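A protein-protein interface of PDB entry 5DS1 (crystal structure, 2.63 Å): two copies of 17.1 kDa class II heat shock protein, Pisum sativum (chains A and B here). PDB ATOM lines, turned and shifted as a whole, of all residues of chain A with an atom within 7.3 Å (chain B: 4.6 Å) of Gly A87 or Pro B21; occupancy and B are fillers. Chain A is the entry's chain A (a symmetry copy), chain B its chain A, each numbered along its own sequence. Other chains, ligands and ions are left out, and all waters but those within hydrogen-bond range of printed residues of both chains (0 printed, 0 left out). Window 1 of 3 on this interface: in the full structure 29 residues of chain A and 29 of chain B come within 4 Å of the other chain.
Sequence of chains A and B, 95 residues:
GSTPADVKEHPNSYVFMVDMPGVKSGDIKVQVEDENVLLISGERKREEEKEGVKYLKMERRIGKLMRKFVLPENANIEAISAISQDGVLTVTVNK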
ATOM      1  N   THR A   3      13.384  14.225   2.629  1.00  0.00           N
ATOM      2  CA  THR A   3      13.977  14.673   3.884  1.00  0.00           C
ATOM      3  C   THR A   3      15.444  15.039   3.680  1.00  0.00           C
ATOM      4  O   THR A   3      16.096  14.491   2.779  1.00  0.00           O
ATOM      5  CB  THR A   3      13.812  13.578   4.946  1.00  0.00           C
ATOM      6  OG1 THR A   3      14.393  13.981   6.203  1.00  0.00           O
ATOM      7  CG2 THR A   3      14.442  12.268   4.462  1.00  0.00           C
ATOM      8  N   PRO A   4      15.995  15.966   4.478  1.00  0.00           N
ATOM      9  CA  PRO A   4      17.358  16.455   4.238  1.00  0.00           C
ATOM     10  C   PRO A   4      18.413  15.358   4.333  1.00  0.00           C
ATOM     11  O   PRO A   4      18.374  14.521   5.235  1.00  0.00           O
ATOM     12  CB  PRO A   4      17.549  17.492   5.350  1.00  0.00           C
ATOM     13  CG  PRO A   4      16.197  17.929   5.663  1.00  0.00           C
ATOM     14  CD  PRO A   4      15.344  16.745   5.547  1.00  0.00           C
ATOM     15  N   VAL A  18      20.917  11.329   7.048  1.00  0.00           N
ATOM     16  CA  VAL A  18      19.537  11.682   6.755  1.00  0.00           C
ATOM     17  C   VAL A  18      18.859  12.137   8.050  1.00  0.00           C
ATOM     18  O   VAL A  18      19.035  11.507   9.093  1.00  0.00           O
ATOM     19  CB  VAL A  18      18.799  10.492   6.121  1.00  0.00           C
ATOM     20  CG1 VAL A  18      17.452  10.922   5.596  1.00  0.00           C
ATOM     21  CG2 VAL A  18      19.667   9.864   5.008  1.00  0.00           C
ATOM     22  N   ASP A  19      18.119  13.252   7.996  1.00  0.00           N
ATOM     23  CA  ASP A  19      17.286  13.636   9.138  1.00  0.00           C
ATOM     24  C   ASP A  19      16.042  12.756   9.215  1.00  0.00           C
ATOM     25  O   ASP A  19      15.337  12.560   8.216  1.00  0.00           O
ATOM     26  CB  ASP A  19      16.862  15.111   9.084  1.00  0.00           C
ATOM     27  CG  ASP A  19      18.036  16.070   9.159  1.00  0.00           C
ATOM     28  OD1 ASP A  19      19.007  15.729   9.857  1.00  0.00           O
ATOM     29  OD2 ASP A  19      18.002  17.152   8.493  1.00  0.00           O
ATOM     30  N   MET A  20      15.761  12.245  10.412  1.00  0.00           N
ATOM     31  CA  MET A  20      14.559  11.454  10.685  1.00  0.00           C
ATOM     32  C   MET A  20      14.142  11.687  12.136  1.00  0.00           C
ATOM     33  O   MET A  20      14.261  10.805  12.984  1.00  0.00           O
ATOM     34  CB  MET A  20      14.814   9.964  10.416  1.00  0.00           C
ATOM     35  CG  MET A  20      15.103   9.658   8.928  1.00  0.00           C
ATOM     36  SD  MET A  20      14.645   8.046   8.301  1.00  0.00           S
ATOM     37  CE  MET A  20      16.229   7.454   7.716  1.00  0.00           C
ATOM     38  N   PRO A  21      13.657  12.885  12.456  1.00  0.00           N
ATOM     39  CA  PRO A  21      13.130  13.085  13.816  1.00  0.00           C
ATOM     40  C   PRO A  21      11.945  12.158  14.035  1.00  0.00           C
ATOM     41  O   PRO A  21      11.136  11.933  13.135  1.00  0.00           O
ATOM     42  CB  PRO A  21      12.717  14.566  13.841  1.00  0.00           C
ATOM     43  CG  PRO A  21      12.633  14.997  12.411  1.00  0.00           C
ATOM     44  CD  PRO A  21      13.513  14.073  11.595  1.00  0.00           C
ATOM     45  N   GLY A  22      11.872  11.569  15.225  1.00  0.00           N
ATOM     46  CA  GLY A  22      10.665  10.842  15.570  1.00  0.00           C
ATOM     47  C   GLY A  22      10.409   9.555  14.811  1.00  0.00           C
ATOM     48  O   GLY A  22       9.261   9.092  14.768  1.00  0.00           O
ATOM     49  N   VAL A  23      11.436   8.945  14.219  1.00  0.00           N
ATOM     50  CA  VAL A  23      11.280   7.651  13.567  1.00  0.00           C
ATOM     51  C   VAL A  23      11.944   6.618  14.445  1.00  0.00           C
ATOM     52  O   VAL A  23      13.142   6.718  14.750  1.00  0.00           O
ATOM     53  CB  VAL A  23      11.866   7.622  12.146  1.00  0.00           C
ATOM     54  CG1 VAL A  23      11.935   6.195  11.662  1.00  0.00           C
ATOM     55  CG2 VAL A  23      11.008   8.426  11.207  1.00  0.00           C
ATOM     56  N   LEU A  65       9.375   9.358   5.328  1.00  0.00           N
ATOM     57  CA  LEU A  65      10.518  10.033   4.730  1.00  0.00           C
ATOM     58  C   LEU A  65      11.275   9.009   3.888  1.00  0.00           C
ATOM     59  O   LEU A  65      11.447   7.864   4.313  1.00  0.00           O
ATOM     60  CB  LEU A  65      11.413  10.599   5.832  1.00  0.00           C
ATOM     61  CG  LEU A  65      10.678  11.306   6.976  1.00  0.00           C
ATOM     62  CD1 LEU A  65      11.636  11.808   8.007  1.00  0.00           C
ATOM     63  CD2 LEU A  65       9.850  12.462   6.480  1.00  0.00           C
ATOM     64  N   ILE A  83      23.572   3.728  11.498  1.00  0.00           N
ATOM     65  CA  ILE A  83      23.477   4.247  12.864  1.00  0.00           C
ATOM     66  C   ILE A  83      22.292   5.190  12.960  1.00  0.00           C
ATOM     67  O   ILE A  83      22.129   6.074  12.119  1.00  0.00           O
ATOM     68  CB  ILE A  83      24.737   5.000  13.331  1.00  0.00           C
ATOM     69  CG1 ILE A  83      25.728   4.059  13.965  1.00  0.00           C
ATOM     70  CG2 ILE A  83      24.368   5.990  14.407  1.00  0.00           C
ATOM     71  CD1 ILE A  83      26.936   4.732  14.411  1.00  0.00           C
ATOM     72  N   SER A  84      21.486   5.013  13.991  1.00  0.00           N
ATOM     73  CA  SER A  84      20.399   5.921  14.319  1.00  0.00           C
ATOM     74  C   SER A  84      20.810   6.673  15.583  1.00  0.00           C
ATOM     75  O   SER A  84      21.128   6.049  16.602  1.00  0.00           O
ATOM     76  CB  SER A  84      19.105   5.129  14.520  1.00  0.00           C
ATOM     77  OG  SER A  84      17.977   5.968  14.664  1.00  0.00           O
ATOM     78  N   GLN A  85      20.844   8.005  15.512  1.00  0.00           N
ATOM     79  CA  GLN A  85      21.189   8.770  16.705  1.00  0.00           C
ATOM     80  C   GLN A  85      20.656  10.192  16.640  1.00  0.00           C
ATOM     81  O   GLN A  85      21.108  10.992  15.813  1.00  0.00           O
ATOM     82  CB  GLN A  85      22.685   8.794  16.913  1.00  0.00           C
ATOM     83  CG  GLN A  85      23.054   9.649  18.098  1.00  0.00           C
ATOM     84  CD  GLN A  85      24.512   9.590  18.404  1.00  0.00           C
ATOM     85  OE1 GLN A  85      25.328   9.252  17.546  1.00  0.00           O
ATOM     86  NE2 GLN A  85      24.860   9.905  19.646  1.00  0.00           N
ATOM     87  N   ASP A  86      19.771  10.523  17.580  1.00  0.00           N
ATOM     88  CA  ASP A  86      19.250  11.878  17.768  1.00  0.00           C
ATOM     89  C   ASP A  86      18.482  12.325  16.551  1.00  0.00           C
ATOM     90  O   ASP A  86      18.508  13.503  16.174  1.00  0.00           O
ATOM     91  CB  ASP A  86      20.355  12.880  18.133  1.00  0.00           C
ATOM     92  CG  ASP A  86      20.959  12.584  19.492  1.00  0.00           C
ATOM     93  OD1 ASP A  86      20.187  12.091  20.341  1.00  0.00           O
ATOM     94  OD2 ASP A  86      22.176  12.820  19.716  1.00  0.00           O
ATOM     95  N   GLY A  87      17.807  11.348  15.946  1.00  0.00           N
ATOM     96  CA  GLY A  87      16.975  11.553  14.783  1.00  0.00           C
ATOM     97  C   GLY A  87      17.735  11.660  13.490  1.00  0.00           C
ATOM     98  O   GLY A  87      17.145  12.052  12.478  1.00  0.00           O
ATOM     99  N   VAL A  88      19.027  11.355  13.485  1.00  0.00           N
ATOM    100  CA  VAL A  88      19.805  11.359  12.258  1.00  0.00           C
ATOM    101  C   VAL A  88      20.276   9.946  11.962  1.00  0.00           C
ATOM    102  O   VAL A  88      20.832   9.261  12.833  1.00  0.00           O
ATOM    103  CB  VAL A  88      20.980  12.334  12.346  1.00  0.00           C
ATOM    104  CG1 VAL A  88      21.782  12.264  11.056  1.00  0.00           C
ATOM    105  CG2 VAL A  88      20.432  13.748  12.545  1.00  0.00           C
ATOM    106  N   LEU A  89      20.040   9.494  10.749  1.00  0.00           N
ATOM    107  CA  LEU A  89      20.483   8.170  10.346  1.00  0.00           C
ATOM    108  C   LEU A  89      21.720   8.312   9.469  1.00  0.00           C
ATOM    109  O   LEU A  89      21.663   8.955   8.412  1.00  0.00           O
ATOM    110  CB  LEU A  89      19.375   7.423   9.609  1.00  0.00           C
ATOM    111  CG  LEU A  89      19.864   6.063   9.122  1.00  0.00           C
ATOM    112  CD1 LEU A  89      19.440   4.958  10.066  1.00  0.00           C
ATOM    113  CD2 LEU A  89      19.370   5.794   7.719  1.00  0.00           C
ATOM    114  N   ASP B  19      10.729  18.965  16.977  1.00  0.00           N
ATOM    115  CA  ASP B  19      11.736  18.253  16.187  1.00  0.00           C
ATOM    116  C   ASP B  19      13.111  18.886  16.376  1.00  0.00           C
ATOM    117  O   ASP B  19      13.271  20.109  16.273  1.00  0.00           O
ATOM    118  CB  ASP B  19      11.392  18.223  14.691  1.00  0.00           C
ATOM    119  CG  ASP B  19      10.107  17.474  14.390  1.00  0.00           C
ATOM    120  OD1 ASP B  19       9.837  16.495  15.109  1.00  0.00           O
ATOM    121  OD2 ASP B  19       9.349  17.883  13.457  1.00  0.00           O
ATOM    122  N   MET B  20      14.111  18.043  16.632  1.00  0.00           N
ATOM    123  CA  MET B  20      15.507  18.469  16.751  1.00  0.00           C
ATOM    124  C   MET B  20      16.406  17.329  16.273  1.00  0.00           C
ATOM    125  O   MET B  20      17.097  16.687  17.061  1.00  0.00           O
ATOM    126  CB  MET B  20      15.836  18.860  18.199  1.00  0.00           C
ATOM    127  CG  MET B  20      15.051  20.101  18.684  1.00  0.00           C
ATOM    128  SD  MET B  20      15.812  21.141  19.925  1.00  0.00           S
ATOM    129  CE  MET B  20      14.580  21.072  21.220  1.00  0.00           C
ATOM    130  N   PRO B  21      16.406  17.046  14.972  1.00  0.00           N
ATOM    131  CA  PRO B  21      17.360  16.040  14.476  1.00  0.00           C
ATOM    132  C   PRO B  21      18.777  16.529  14.727  1.00  0.00           C
ATOM    133  O   PRO B  21      19.075  17.716  14.594  1.00  0.00           O
ATOM    134  CB  PRO B  21      17.043  15.934  12.975  1.00  0.00           C
ATOM    135  CG  PRO B  21      16.249  17.155  12.632  1.00  0.00           C
ATOM    136  CD  PRO B  21      15.593  17.655  13.903  1.00  0.00           C
ATOM    137  N   GLY B  22      19.648  15.617  15.149  1.00  0.00           N
ATOM    138  CA  GLY B  22      21.054  15.969  15.205  1.00  0.00           C
ATOM    139  C   GLY B  22      21.457  16.980  16.261  1.00  0.00           C
ATOM    140  O   GLY B  22      22.521  17.602  16.134  1.00  0.00           O
ATOM    141  N   VAL B  23      20.657  17.163  17.312  1.00  0.00           N
ATOM    142  CA  VAL B  23      21.036  18.036  18.415  1.00  0.00           C
ATOM    143  C   VAL B  23      21.389  17.156  19.589  1.00  0.00           C
ATOM    144  O   VAL B  23      20.568  16.347  20.047  1.00  0.00           O
ATOM    145  CB  VAL B  23      19.933  19.039  18.790  1.00  0.00           C
ATOM    146  CG1 VAL B  23      20.276  19.690  20.107  1.00  0.00           C
ATOM    147  CG2 VAL B  23      19.801  20.098  17.730  1.00  0.00           C
ATOM    148  N   ARG B  44      22.233  22.428  16.031  1.00  0.00           N
ATOM    149  CA  ARG B  44      22.884  21.354  15.290  1.00  0.00           C
ATOM    150  C   ARG B  44      24.239  21.829  14.785  1.00  0.00           C
ATOM    151  O   ARG B  44      24.367  22.945  14.256  1.00  0.00           O
ATOM    152  CB  ARG B  44      22.033  20.880  14.107  1.00  0.00           C
ATOM    153  CG  ARG B  44      20.547  21.148  14.220  1.00  0.00           C
ATOM    154  CD  ARG B  44      19.893  21.054  12.864  1.00  0.00           C
ATOM    155  NE  ARG B  44      19.793  19.665  12.438  1.00  0.00           N
ATOM    156  CZ  ARG B  44      19.776  19.260  11.172  1.00  0.00           C
ATOM    157  NH1 ARG B  44      19.869  20.135  10.183  1.00  0.00           N
ATOM    158  NH2 ARG B  44      19.675  17.969  10.899  1.00  0.00           N
ATOM    159  N   ASP B  86      15.140  10.280  19.644  1.00  0.00           N
ATOM    160  CA  ASP B  86      15.037  10.099  18.196  1.00  0.00           C
ATOM    161  C   ASP B  86      14.862  11.428  17.507  1.00  0.00           C
ATOM    162  O   ASP B  86      14.151  11.539  16.500  1.00  0.00           O
ATOM    163  CB  ASP B  86      13.922   9.116  17.810  1.00  0.00           C
ATOM    164  CG  ASP B  86      14.224   7.707  18.281  1.00  0.00           C
ATOM    165  OD1 ASP B  86      15.430   7.383  18.310  1.00  0.00           O
ATOM    166  OD2 ASP B  86      13.290   6.937  18.631  1.00  0.00           O
ATOM    167  N   GLY B  87      15.523  12.431  18.085  1.00  0.00           N
ATOM    168  CA  GLY B  87      15.528  13.782  17.576  1.00  0.00           C
ATOM    169  C   GLY B  87      14.291  14.572  17.908  1.00  0.00           C
ATOM    170  O   GLY B  87      14.100  15.652  17.339  1.00  0.00           O
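Among the printed residues, merely in contact across the chains: Asp A19 with Pro B21 (3.7 Å), Met A20 with Asp B86 (3.6 Å), Pro A21 with Asp B19 (3.7 Å), Pro A21 with Asp B86 (3.3 Å), Pro A21 with Gly B87 (3.9 Å), Val A23 with Asp B86 (3.8 Å), Asp A86 with Met B20 (3.6 Å), Asp A86 with Pro B21 (3.3 Å), Asp A86 with Val B23 (3.8 Å), Asp A86 with Asp B86 (3.9 Å), Asp A86 with Gly B87 (3.3 Å), Gly A87 with Pro B21 (3.9 Å), Gly A87 with Asp B86 (3.3 Å), Val A88 with Pro B21 (3.9 Å) and Val A88 with Gly B22 (3.3 Å).
The backbone NH of Gly B22 sits at hydrogen-bond distance from the backbone carbonyl oxygen of Asp A86 (2.6 Å).
OD1 of Asp A19 lies within salt-bridge range of NH2 of Arg B44 (2.6 Å).
The backbone carbonyl oxygen of Asp B86 sits at hydrogen-bond distance from the backbone NH of Gly A22 (2.6 Å).
The backbone NH (N) of Gly B87 lies close to the backbone NH (N) of Gly A87, at 3.3 Å.
The backbone carbonyl oxygen (O) of Gly B87 is in hydrogen-bond range of the backbone NH (N) of Met B20 (2.5 Å).
The backbone carbonyl oxygen of Pro B21 lies within hydrogen-bond range of the guanidinium group of Arg B44 (3.0 Å).
The side-chain hydroxyl of Thr A3 sits at hydrogen-bond distance from the backbone carbonyl oxygen of Asp A19, at 2.6 Å.
The backbone carbonyl oxygen (O) of Pro A4 is in hydrogen-bond range of the backbone NH (N) of Asp A19 (3.0 Å).
The backbone carbonyl oxygen (O) of Gly A87 sits at hydrogen-bond distance from the backbone NH (N) of Met A20 (2.5 Å).
Met A20 touches Asp B86, and with the chains exchanged Asp A86 touches Met B20.
Val A23 touches Asp B86, and with the chains exchanged Asp A86 touches Val B23.
Asp B86 touches its own counterpart, Asp A86.
Gly A87 touches its own counterpart, Gly B87.
Of the printed residues of chain B, Met A20 touches Asp B86 (3.6 Å).
Printed residues of chain B within 4 Å of Gly A22: Asp B86 (2.6 Å).
Gly A87 touches three residues of chain B.
Of the printed residues of chain B, Val A88 touches Pro B21 (3.9 Å) and Gly B22 (3.3 Å).
Pro B21 touches four residues of chain A.
Of the printed residues of chain A, Asp B86 touches Met A20, Pro A21, Gly A22, Val A23, Asp A86 and Gly A87.
The nearest printed residue of chain B that does not touch Gly A87 is Gly B22 (4.7 Å).
The nearest residue of chain A that does not touch Pro B21 is Pro A21 (4.2 Å).
Hydrophobic or aromatic side chains of chain A within 4 Å of the printed part of chain B: Pro A21 and Val A88.
Of the 8 printed residues of chain B, 8 touch a printed residue of chain A.
Printed residues of chain B that touch a printed residue of chain A: Asp B19, Met B20, Pro B21, Gly B22, Val B23, Arg B44, Asp B86 and Gly B87.
Among the printed residues, 19 pairs touch across the chains.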
